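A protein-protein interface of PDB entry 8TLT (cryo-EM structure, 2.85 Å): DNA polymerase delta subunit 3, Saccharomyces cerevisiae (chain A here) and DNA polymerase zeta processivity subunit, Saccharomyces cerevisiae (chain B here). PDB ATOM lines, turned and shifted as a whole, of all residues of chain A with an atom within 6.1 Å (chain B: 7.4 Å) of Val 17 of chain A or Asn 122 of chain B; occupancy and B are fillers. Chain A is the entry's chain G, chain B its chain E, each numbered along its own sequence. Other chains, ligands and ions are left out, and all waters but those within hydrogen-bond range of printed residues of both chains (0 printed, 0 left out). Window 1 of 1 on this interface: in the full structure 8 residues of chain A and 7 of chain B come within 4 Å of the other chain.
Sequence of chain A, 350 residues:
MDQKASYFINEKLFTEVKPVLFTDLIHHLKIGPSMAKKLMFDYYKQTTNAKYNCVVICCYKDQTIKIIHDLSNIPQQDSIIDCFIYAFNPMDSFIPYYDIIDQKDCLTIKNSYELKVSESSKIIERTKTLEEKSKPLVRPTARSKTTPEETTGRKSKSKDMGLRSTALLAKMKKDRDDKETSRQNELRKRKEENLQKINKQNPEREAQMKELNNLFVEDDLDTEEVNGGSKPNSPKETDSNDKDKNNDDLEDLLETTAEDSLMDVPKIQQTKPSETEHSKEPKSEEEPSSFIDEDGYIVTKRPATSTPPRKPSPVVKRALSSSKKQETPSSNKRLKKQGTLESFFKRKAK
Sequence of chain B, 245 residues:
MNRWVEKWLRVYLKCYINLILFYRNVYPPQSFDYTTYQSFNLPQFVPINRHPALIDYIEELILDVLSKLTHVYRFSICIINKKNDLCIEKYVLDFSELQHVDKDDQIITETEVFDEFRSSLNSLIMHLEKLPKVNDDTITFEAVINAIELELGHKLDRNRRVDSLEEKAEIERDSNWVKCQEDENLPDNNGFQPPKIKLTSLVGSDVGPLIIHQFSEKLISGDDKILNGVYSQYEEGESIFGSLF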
ATOM      1  N   GLU A  11     -11.743  -6.603 -20.981  1.00  0.00           N
ATOM      2  CA  GLU A  11     -12.587  -7.219 -19.963  1.00  0.00           C
ATOM      3  C   GLU A  11     -13.631  -8.131 -20.597  1.00  0.00           C
ATOM      4  O   GLU A  11     -13.729  -9.313 -20.249  1.00  0.00           O
ATOM      5  CB  GLU A  11     -13.258  -6.138 -19.117  1.00  0.00           C
ATOM      6  CG  GLU A  11     -13.733  -6.616 -17.757  1.00  0.00           C
ATOM      7  CD  GLU A  11     -12.644  -6.553 -16.706  1.00  0.00           C
ATOM      8  N   LYS A  12     -14.392  -7.606 -21.561  1.00  0.00           N
ATOM      9  CA  LYS A  12     -15.464  -8.367 -22.192  1.00  0.00           C
ATOM     10  C   LYS A  12     -14.954  -9.502 -23.068  1.00  0.00           C
ATOM     11  O   LYS A  12     -15.754 -10.347 -23.479  1.00  0.00           O
ATOM     12  CB  LYS A  12     -16.343  -7.433 -23.024  1.00  0.00           C
ATOM     13  CG  LYS A  12     -17.826  -7.757 -22.972  1.00  0.00           C
ATOM     14  CD  LYS A  12     -18.378  -8.027 -24.362  1.00  0.00           C
ATOM     15  CE  LYS A  12     -19.845  -8.419 -24.305  1.00  0.00           C
ATOM     16  NZ  LYS A  12     -20.443  -8.522 -25.664  1.00  0.00           N
ATOM     17  N   LEU A  13     -13.659  -9.535 -23.375  1.00  0.00           N
ATOM     18  CA  LEU A  13     -13.085 -10.611 -24.168  1.00  0.00           C
ATOM     19  C   LEU A  13     -12.416 -11.688 -23.329  1.00  0.00           C
ATOM     20  O   LEU A  13     -12.419 -12.856 -23.728  1.00  0.00           O
ATOM     21  CB  LEU A  13     -12.059 -10.043 -25.154  1.00  0.00           C
ATOM     22  CG  LEU A  13     -12.015 -10.607 -26.574  1.00  0.00           C
ATOM     23  CD1 LEU A  13     -13.398 -11.037 -27.030  1.00  0.00           C
ATOM     24  CD2 LEU A  13     -11.427  -9.583 -27.529  1.00  0.00           C
ATOM     25  N   PHE A  14     -11.846 -11.332 -22.181  1.00  0.00           N
ATOM     26  CA  PHE A  14     -11.069 -12.286 -21.400  1.00  0.00           C
ATOM     27  C   PHE A  14     -11.634 -12.552 -20.015  1.00  0.00           C
ATOM     28  O   PHE A  14     -11.670 -13.709 -19.589  1.00  0.00           O
ATOM     29  CB  PHE A  14      -9.621 -11.795 -21.284  1.00  0.00           C
ATOM     30  CG  PHE A  14      -8.947 -11.595 -22.611  1.00  0.00           C
ATOM     31  CD1 PHE A  14      -9.123 -12.510 -23.634  1.00  0.00           C
ATOM     32  CD2 PHE A  14      -8.156 -10.485 -22.842  1.00  0.00           C
ATOM     33  CE1 PHE A  14      -8.514 -12.327 -24.858  1.00  0.00           C
ATOM     34  CE2 PHE A  14      -7.543 -10.298 -24.065  1.00  0.00           C
ATOM     35  CZ  PHE A  14      -7.723 -11.220 -25.074  1.00  0.00           C
ATOM     36  N   THR A  15     -12.066 -11.517 -19.287  1.00  0.00           N
ATOM     37  CA  THR A  15     -12.646 -11.750 -17.968  1.00  0.00           C
ATOM     38  C   THR A  15     -13.923 -12.571 -18.076  1.00  0.00           C
ATOM     39  O   THR A  15     -14.135 -13.513 -17.304  1.00  0.00           O
ATOM     40  CB  THR A  15     -12.919 -10.418 -17.269  1.00  0.00           C
ATOM     41  OG1 THR A  15     -11.687  -9.701 -17.109  1.00  0.00           O
ATOM     42  CG2 THR A  15     -13.545 -10.650 -15.904  1.00  0.00           C
ATOM     43  N   GLU A  16     -14.781 -12.230 -19.031  1.00  0.00           N
ATOM     44  CA  GLU A  16     -15.930 -13.041 -19.401  1.00  0.00           C
ATOM     45  C   GLU A  16     -15.814 -13.364 -20.881  1.00  0.00           C
ATOM     46  O   GLU A  16     -15.625 -12.461 -21.701  1.00  0.00           O
ATOM     47  CB  GLU A  16     -17.243 -12.314 -19.108  1.00  0.00           C
ATOM     48  CG  GLU A  16     -17.201 -10.826 -19.397  1.00  0.00           C
ATOM     49  CD  GLU A  16     -18.348 -10.074 -18.756  1.00  0.00           C
ATOM     50  OE1 GLU A  16     -19.514 -10.363 -19.097  1.00  0.00           O
ATOM     51  OE2 GLU A  16     -18.084  -9.192 -17.912  1.00  0.00           O
ATOM     52  N   VAL A  17     -15.919 -14.644 -21.225  1.00  0.00           N
ATOM     53  CA  VAL A  17     -15.715 -15.057 -22.607  1.00  0.00           C
ATOM     54  C   VAL A  17     -16.966 -14.729 -23.408  1.00  0.00           C
ATOM     55  O   VAL A  17     -17.914 -15.519 -23.456  1.00  0.00           O
ATOM     56  CB  VAL A  17     -15.366 -16.553 -22.700  1.00  0.00           C
ATOM     57  CG1 VAL A  17     -14.961 -16.912 -24.118  1.00  0.00           C
ATOM     58  CG2 VAL A  17     -14.254 -16.894 -21.726  1.00  0.00           C
ATOM     59  N   LYS A  18     -16.974 -13.556 -24.039  1.00  0.00           N
ATOM     60  CA  LYS A  18     -18.094 -13.082 -24.831  1.00  0.00           C
ATOM     61  C   LYS A  18     -17.541 -12.354 -26.047  1.00  0.00           C
ATOM     62  O   LYS A  18     -16.567 -11.598 -25.923  1.00  0.00           O
ATOM     63  CB  LYS A  18     -19.002 -12.132 -24.036  1.00  0.00           C
ATOM     64  CG  LYS A  18     -19.588 -12.719 -22.761  1.00  0.00           C
ATOM     65  CD  LYS A  18     -20.815 -13.561 -23.046  1.00  0.00           C
ATOM     66  CE  LYS A  18     -21.437 -14.071 -21.758  1.00  0.00           C
ATOM     67  NZ  LYS A  18     -21.881 -12.956 -20.879  1.00  0.00           N
ATOM     68  N   PRO A  19     -18.120 -12.568 -27.225  1.00  0.00           N
ATOM     69  CA  PRO A  19     -17.721 -11.769 -28.387  1.00  0.00           C
ATOM     70  C   PRO A  19     -18.027 -10.297 -28.161  1.00  0.00           C
ATOM     71  O   PRO A  19     -19.031  -9.940 -27.539  1.00  0.00           O
ATOM     72  CB  PRO A  19     -18.556 -12.355 -29.531  1.00  0.00           C
ATOM     73  CG  PRO A  19     -19.685 -13.063 -28.863  1.00  0.00           C
ATOM     74  CD  PRO A  19     -19.148 -13.566 -27.563  1.00  0.00           C
ATOM     75  N   PRO A  90     -13.381 -14.669 -29.282  1.00  0.00           N
ATOM     76  CA  PRO A  90     -12.354 -15.476 -28.616  1.00  0.00           C
ATOM     77  C   PRO A  90     -12.376 -16.946 -29.001  1.00  0.00           C
ATOM     78  O   PRO A  90     -11.519 -17.702 -28.531  1.00  0.00           O
ATOM     79  CB  PRO A  90     -12.682 -15.299 -27.123  1.00  0.00           C
ATOM     80  CG  PRO A  90     -14.020 -14.608 -27.055  1.00  0.00           C
ATOM     81  CD  PRO A  90     -14.567 -14.474 -28.435  1.00  0.00           C
ATOM     82  N   MET A  91     -13.321 -17.370 -29.837  1.00  0.00           N
ATOM     83  CA  MET A  91     -13.483 -18.773 -30.188  1.00  0.00           C
ATOM     84  C   MET A  91     -13.772 -18.885 -31.677  1.00  0.00           C
ATOM     85  O   MET A  91     -14.041 -17.892 -32.357  1.00  0.00           O
ATOM     86  CB  MET A  91     -14.605 -19.417 -29.371  1.00  0.00           C
ATOM     87  CG  MET A  91     -15.687 -18.436 -28.976  1.00  0.00           C
ATOM     88  SD  MET A  91     -16.922 -19.122 -27.866  1.00  0.00           S
ATOM     89  CE  MET A  91     -17.413 -17.634 -27.006  1.00  0.00           C
ATOM     90  N   LEU B  19     -21.822 -30.702 -24.515  1.00  0.00           N
ATOM     91  CA  LEU B  19     -20.676 -30.039 -25.129  1.00  0.00           C
ATOM     92  C   LEU B  19     -19.439 -30.925 -25.086  1.00  0.00           C
ATOM     93  O   LEU B  19     -18.699 -31.019 -26.074  1.00  0.00           O
ATOM     94  CB  LEU B  19     -20.403 -28.710 -24.427  1.00  0.00           C
ATOM     95  CG  LEU B  19     -21.260 -27.518 -24.850  1.00  0.00           C
ATOM     96  CD1 LEU B  19     -21.074 -26.362 -23.883  1.00  0.00           C
ATOM     97  CD2 LEU B  19     -20.924 -27.096 -26.270  1.00  0.00           C
ATOM     98  N   GLN B  44     -27.535 -20.943 -24.488  1.00  0.00           N
ATOM     99  CA  GLN B  44     -27.093 -20.590 -25.835  1.00  0.00           C
ATOM    100  C   GLN B  44     -27.607 -21.655 -26.796  1.00  0.00           C
ATOM    101  O   GLN B  44     -28.480 -22.462 -26.461  1.00  0.00           O
ATOM    102  CB  GLN B  44     -25.563 -20.471 -25.925  1.00  0.00           C
ATOM    103  CG  GLN B  44     -24.864 -19.988 -24.682  1.00  0.00           C
ATOM    104  CD  GLN B  44     -23.460 -20.534 -24.569  1.00  0.00           C
ATOM    105  OE1 GLN B  44     -23.211 -21.484 -23.831  1.00  0.00           O
ATOM    106  NE2 GLN B  44     -22.530 -19.937 -25.303  1.00  0.00           N
ATOM    107  N   ASP B 115     -26.622 -15.585 -17.838  1.00  0.00           N
ATOM    108  CA  ASP B 115     -25.429 -14.862 -18.274  1.00  0.00           C
ATOM    109  C   ASP B 115     -24.165 -15.519 -17.731  1.00  0.00           C
ATOM    110  O   ASP B 115     -23.182 -15.717 -18.460  1.00  0.00           O
ATOM    111  CB  ASP B 115     -25.510 -13.402 -17.827  1.00  0.00           C
ATOM    112  CG  ASP B 115     -26.174 -12.512 -18.855  1.00  0.00           C
ATOM    113  N   GLU B 116     -24.179 -15.873 -16.443  1.00  0.00           N
ATOM    114  CA  GLU B 116     -23.033 -16.569 -15.863  1.00  0.00           C
ATOM    115  C   GLU B 116     -22.820 -17.923 -16.530  1.00  0.00           C
ATOM    116  O   GLU B 116     -21.679 -18.321 -16.805  1.00  0.00           O
ATOM    117  CB  GLU B 116     -23.226 -16.739 -14.356  1.00  0.00           C
ATOM    118  CG  GLU B 116     -22.762 -15.552 -13.528  1.00  0.00           C
ATOM    119  CD  GLU B 116     -21.271 -15.301 -13.634  1.00  0.00           C
ATOM    120  OE1 GLU B 116     -20.520 -16.255 -13.923  1.00  0.00           O
ATOM    121  OE2 GLU B 116     -20.847 -14.146 -13.425  1.00  0.00           O
ATOM    122  N   PHE B 117     -23.911 -18.645 -16.799  1.00  0.00           N
ATOM    123  CA  PHE B 117     -23.807 -19.928 -17.481  1.00  0.00           C
ATOM    124  C   PHE B 117     -23.238 -19.759 -18.881  1.00  0.00           C
ATOM    125  O   PHE B 117     -22.443 -20.586 -19.339  1.00  0.00           O
ATOM    126  CB  PHE B 117     -25.178 -20.604 -17.541  1.00  0.00           C
ATOM    127  CG  PHE B 117     -25.615 -21.210 -16.239  1.00  0.00           C
ATOM    128  CD1 PHE B 117     -24.789 -21.178 -15.129  1.00  0.00           C
ATOM    129  CD2 PHE B 117     -26.852 -21.819 -16.128  1.00  0.00           C
ATOM    130  CE1 PHE B 117     -25.190 -21.737 -13.934  1.00  0.00           C
ATOM    131  CE2 PHE B 117     -27.258 -22.378 -14.935  1.00  0.00           C
ATOM    132  CZ  PHE B 117     -26.426 -22.337 -13.837  1.00  0.00           C
ATOM    133  N   ARG B 118     -23.644 -18.697 -19.580  1.00  0.00           N
ATOM    134  CA  ARG B 118     -23.112 -18.430 -20.909  1.00  0.00           C
ATOM    135  C   ARG B 118     -21.614 -18.183 -20.854  1.00  0.00           C
ATOM    136  O   ARG B 118     -20.863 -18.705 -21.681  1.00  0.00           O
ATOM    137  CB  ARG B 118     -23.829 -17.230 -21.527  1.00  0.00           C
ATOM    138  CG  ARG B 118     -25.137 -17.574 -22.207  1.00  0.00           C
ATOM    139  CD  ARG B 118     -25.530 -16.521 -23.225  1.00  0.00           C
ATOM    140  NE  ARG B 118     -25.853 -15.248 -22.593  1.00  0.00           N
ATOM    141  CZ  ARG B 118     -27.028 -14.961 -22.049  1.00  0.00           C
ATOM    142  NH1 ARG B 118     -28.018 -15.838 -22.042  1.00  0.00           N
ATOM    143  NH2 ARG B 118     -27.214 -13.764 -21.503  1.00  0.00           N
ATOM    144  N   SER B 119     -21.160 -17.403 -19.871  1.00  0.00           N
ATOM    145  CA  SER B 119     -19.725 -17.163 -19.736  1.00  0.00           C
ATOM    146  C   SER B 119     -18.967 -18.459 -19.454  1.00  0.00           C
ATOM    147  O   SER B 119     -17.925 -18.727 -20.068  1.00  0.00           O
ATOM    148  CB  SER B 119     -19.469 -16.138 -18.632  1.00  0.00           C
ATOM    149  OG  SER B 119     -18.084 -15.906 -18.466  1.00  0.00           O
ATOM    150  N   SER B 120     -19.488 -19.284 -18.542  1.00  0.00           N
ATOM    151  CA  SER B 120     -18.804 -20.527 -18.186  1.00  0.00           C
ATOM    152  C   SER B 120     -18.749 -21.492 -19.366  1.00  0.00           C
ATOM    153  O   SER B 120     -17.702 -22.089 -19.654  1.00  0.00           O
ATOM    154  CB  SER B 120     -19.502 -21.178 -16.993  1.00  0.00           C
ATOM    155  OG  SER B 120     -19.161 -20.522 -15.787  1.00  0.00           O
ATOM    156  N   LEU B 121     -19.873 -21.656 -20.066  1.00  0.00           N
ATOM    157  CA  LEU B 121     -19.906 -22.561 -21.208  1.00  0.00           C
ATOM    158  C   LEU B 121     -19.061 -22.037 -22.358  1.00  0.00           C
ATOM    159  O   LEU B 121     -18.475 -22.829 -23.100  1.00  0.00           O
ATOM    160  CB  LEU B 121     -21.347 -22.782 -21.661  1.00  0.00           C
ATOM    161  CG  LEU B 121     -22.277 -23.503 -20.682  1.00  0.00           C
ATOM    162  CD1 LEU B 121     -23.676 -23.602 -21.260  1.00  0.00           C
ATOM    163  CD2 LEU B 121     -21.742 -24.882 -20.336  1.00  0.00           C
ATOM    164  N   ASN B 122     -18.985 -20.715 -22.525  1.00  0.00           N
ATOM    165  CA  ASN B 122     -18.104 -20.149 -23.538  1.00  0.00           C
ATOM    166  C   ASN B 122     -16.646 -20.438 -23.214  1.00  0.00           C
ATOM    167  O   ASN B 122     -15.856 -20.757 -24.110  1.00  0.00           O
ATOM    168  CB  ASN B 122     -18.346 -18.647 -23.652  1.00  0.00           C
ATOM    169  CG  ASN B 122     -19.568 -18.316 -24.483  1.00  0.00           C
ATOM    170  OD1 ASN B 122     -20.142 -19.186 -25.137  1.00  0.00           O
ATOM    171  ND2 ASN B 122     -19.971 -17.052 -24.465  1.00  0.00           N
ATOM    172  N   SER B 123     -16.269 -20.329 -21.938  1.00  0.00           N
ATOM    173  CA  SER B 123     -14.914 -20.702 -21.544  1.00  0.00           C
ATOM    174  C   SER B 123     -14.645 -22.173 -21.837  1.00  0.00           C
ATOM    175  O   SER B 123     -13.574 -22.531 -22.350  1.00  0.00           O
ATOM    176  CB  SER B 123     -14.696 -20.403 -20.061  1.00  0.00           C
ATOM    177  OG  SER B 123     -13.319 -20.272 -19.766  1.00  0.00           O
ATOM    178  N   LEU B 124     -15.612 -23.041 -21.525  1.00  0.00           N
ATOM    179  CA  LEU B 124     -15.449 -24.463 -21.809  1.00  0.00           C
ATOM    180  C   LEU B 124     -15.273 -24.718 -23.301  1.00  0.00           C
ATOM    181  O   LEU B 124     -14.409 -25.504 -23.705  1.00  0.00           O
ATOM    182  CB  LEU B 124     -16.646 -25.251 -21.281  1.00  0.00           C
ATOM    183  CG  LEU B 124     -16.622 -26.745 -21.612  1.00  0.00           C
ATOM    184  CD1 LEU B 124     -15.491 -27.449 -20.877  1.00  0.00           C
ATOM    185  CD2 LEU B 124     -17.960 -27.396 -21.310  1.00  0.00           C
ATOM    186  N   ILE B 125     -16.088 -24.068 -24.133  1.00  0.00           N
ATOM    187  CA  ILE B 125     -16.002 -24.265 -25.577  1.00  0.00           C
ATOM    188  C   ILE B 125     -14.667 -23.761 -26.109  1.00  0.00           C
ATOM    189  O   ILE B 125     -14.038 -24.404 -26.961  1.00  0.00           O
ATOM    190  CB  ILE B 125     -17.189 -23.579 -26.277  1.00  0.00           C
ATOM    191  CG1 ILE B 125     -18.489 -24.320 -25.968  1.00  0.00           C
ATOM    192  CG2 ILE B 125     -16.965 -23.514 -27.776  1.00  0.00           C
ATOM    193  CD1 ILE B 125     -19.722 -23.459 -26.093  1.00  0.00           C
ATOM    194  N   MET B 126     -14.211 -22.605 -25.620  1.00  0.00           N
ATOM    195  CA  MET B 126     -12.924 -22.072 -26.056  1.00  0.00           C
ATOM    196  C   MET B 126     -11.789 -23.019 -25.694  1.00  0.00           C
ATOM    197  O   MET B 126     -10.857 -23.210 -26.484  1.00  0.00           O
ATOM    198  CB  MET B 126     -12.692 -20.692 -25.440  1.00  0.00           C
ATOM    199  CG  MET B 126     -11.399 -20.028 -25.880  1.00  0.00           C
ATOM    200  SD  MET B 126     -10.978 -18.584 -24.887  1.00  0.00           S
ATOM    201  CE  MET B 126     -11.297 -19.201 -23.238  1.00  0.00           C
ATOM    202  N   HIS B 127     -11.841 -23.615 -24.501  1.00  0.00           N
ATOM    203  CA  HIS B 127     -10.833 -24.608 -24.141  1.00  0.00           C
ATOM    204  C   HIS B 127     -10.925 -25.846 -25.027  1.00  0.00           C
ATOM    205  O   HIS B 127      -9.899 -26.377 -25.468  1.00  0.00           O
ATOM    206  CB  HIS B 127     -10.973 -25.000 -22.674  1.00  0.00           C
ATOM    207  CG  HIS B 127     -10.091 -26.141 -22.270  1.00  0.00           C
ATOM    208  ND1 HIS B 127      -8.772 -26.235 -22.656  1.00  0.00           N
ATOM    209  CD2 HIS B 127     -10.344 -27.241 -21.522  1.00  0.00           C
ATOM    210  CE1 HIS B 127      -8.247 -27.340 -22.158  1.00  0.00           C
ATOM    211  NE2 HIS B 127      -9.180 -27.969 -21.467  1.00  0.00           N
ATOM    212  N   LEU B 128     -12.143 -26.320 -25.299  1.00  0.00           N
ATOM    213  CA  LEU B 128     -12.313 -27.575 -26.026  1.00  0.00           C
ATOM    214  C   LEU B 128     -11.915 -27.452 -27.490  1.00  0.00           C
ATOM    215  O   LEU B 128     -11.450 -28.431 -28.084  1.00  0.00           O
ATOM    216  CB  LEU B 128     -13.760 -28.054 -25.919  1.00  0.00           C
ATOM    217  CG  LEU B 128     -14.200 -28.651 -24.584  1.00  0.00           C
ATOM    218  CD1 LEU B 128     -15.686 -28.955 -24.608  1.00  0.00           C
ATOM    219  CD2 LEU B 128     -13.401 -29.899 -24.261  1.00  0.00           C
ATOM    220  N   GLU B 129     -12.103 -26.276 -28.092  1.00  0.00           N
ATOM    221  CA  GLU B 129     -11.797 -26.118 -29.511  1.00  0.00           C
ATOM    222  C   GLU B 129     -10.309 -26.299 -29.784  1.00  0.00           C
ATOM    223  O   GLU B 129      -9.924 -26.871 -30.811  1.00  0.00           O
ATOM    224  CB  GLU B 129     -12.269 -24.752 -30.001  1.00  0.00           C
ATOM    225  CG  GLU B 129     -13.762 -24.662 -30.244  1.00  0.00           C
ATOM    226  CD  GLU B 129     -14.224 -23.237 -30.451  1.00  0.00           C
ATOM    227  OE1 GLU B 129     -13.407 -22.314 -30.251  1.00  0.00           O
ATOM    228  OE2 GLU B 129     -15.402 -23.037 -30.813  1.00  0.00           O
ATOM    229  N   LEU B 202     -10.460 -23.084 -15.733  1.00  0.00           N
ATOM    230  CA  LEU B 202     -11.479 -22.455 -16.556  1.00  0.00           C
ATOM    231  C   LEU B 202     -12.354 -21.558 -15.691  1.00  0.00           C
ATOM    232  O   LEU B 202     -12.343 -21.640 -14.460  1.00  0.00           O
ATOM    233  CB  LEU B 202     -12.341 -23.503 -17.273  1.00  0.00           C
ATOM    234  CG  LEU B 202     -11.668 -24.293 -18.395  1.00  0.00           C
ATOM    235  CD1 LEU B 202     -11.088 -25.585 -17.864  1.00  0.00           C
ATOM    236  CD2 LEU B 202     -12.662 -24.579 -19.493  1.00  0.00           C
ATOM    237  N   VAL B 203     -13.121 -20.690 -16.354  1.00  0.00           N
ATOM    238  CA  VAL B 203     -14.014 -19.795 -15.628  1.00  0.00           C
ATOM    239  C   VAL B 203     -15.219 -20.571 -15.107  1.00  0.00           C
ATOM    240  O   VAL B 203     -15.606 -21.617 -15.640  1.00  0.00           O
ATOM    241  CB  VAL B 203     -14.451 -18.619 -16.516  1.00  0.00           C
ATOM    242  N   GLN B 214     -14.721 -24.784 -12.202  1.00  0.00           N
ATOM    243  CA  GLN B 214     -14.524 -25.774 -13.250  1.00  0.00           C
ATOM    244  C   GLN B 214     -13.079 -25.751 -13.722  1.00  0.00           C
ATOM    245  O   GLN B 214     -12.476 -24.684 -13.859  1.00  0.00           O
ATOM    246  CB  GLN B 214     -15.486 -25.522 -14.419  1.00  0.00           C
ATOM    247  CG  GLN B 214     -14.906 -25.769 -15.795  1.00  0.00           C
ATOM    248  CD  GLN B 214     -15.708 -25.092 -16.883  1.00  0.00           C
ATOM    249  OE1 GLN B 214     -16.397 -24.105 -16.635  1.00  0.00           O
ATOM    250  NE2 GLN B 214     -15.627 -25.622 -18.094  1.00  0.00           N
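The backbone carbonyl oxygen (O) of Val 17 of chain A sits at hydrogen-bond distance from the side-chain amide nitrogen (ND2) of Asn 122 of chain B, 2.8 Å away.
The side-chain sulfur of Met 126 of chain B sits close to the backbone carbonyl oxygen of Pro 90 of chain A (3.8 Å).
CA of Glu 16 of chain A touches OG of Ser 119 of chain B (3.7 Å).
Val 17 of chain A touches Ser 119 of chain B (N to OG, 3.7 Å).
Val 17 of chain A touches Ser 123 of chain B (CG2 to CA, 3.9 Å).
Lys 18 of chain A touches Asp 115 of chain B.
CB of Arg 118 of chain B touches CE of Lys 18 of chain A, 3.97 Å away.
Lys 18 of chain A touches Ser 119 of chain B (CE to N, 3.8 Å).
ND2 of Asn 122 of chain B touches CD of Lys 18 of chain A (3.9 Å).
CE of Met 91 of chain A touches CG of Asn 122 of chain B (3.4 Å).
Met 91 of chain A touches Glu 129 of chain B (CB to OE1, 3.3 Å).
Printed residues of chain A within 4 Å of Asn 122 of chain B: Val 17, Lys 18 and Met 91.
Of the printed residues of chain B, Met 91 of chain A touches Asn 122 and Glu 129.
Of the printed residues of chain B, Glu 16 of chain A touches Ser 119.
Glu 11 of chain A touches none of the printed residues of chain B.
The nearest residue of chain A that does not touch Asn 122 of chain B is Pro 19 of chain A (4.7 Å).
Hydrophobic or aromatic side chains of chain A within 4 Å of the printed part of chain B: Val 17 and Met 91.
Of the 20 printed residues of chain B, 7 touch a printed residue of chain A.
Hydrophobic or aromatic side chains of chain B that line the printed part of chain A: Met 126.
NE2 of Gln 44 of chain B sits at hydrogen-bond distance from OD1 of Asn 122 of chain B, 2.5 Å away.
N of Val 203 of chain B is in hydrogen-bond range of OG of Ser 123 of chain B (3.4 Å).
N of Lys 18 of chain A lies within hydrogen-bond range of O of Lys 12 of chain A (3.5 Å).
The backbone carbonyl oxygen of Arg 118 of chain B sits close to the side-chain amide nitrogen of Asn 122 of chain B (3.4 Å).
The backbone NH (N) of Glu 16 of chain A sits at hydrogen-bond distance from the backbone carbonyl oxygen (O) of Glu 11 of chain A (3.3 Å).
The side-chain amino group of Lys 18 of chain A is in salt-bridge range of the side-chain carboxylate of Glu 16 of chain A, 3.9 Å away.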
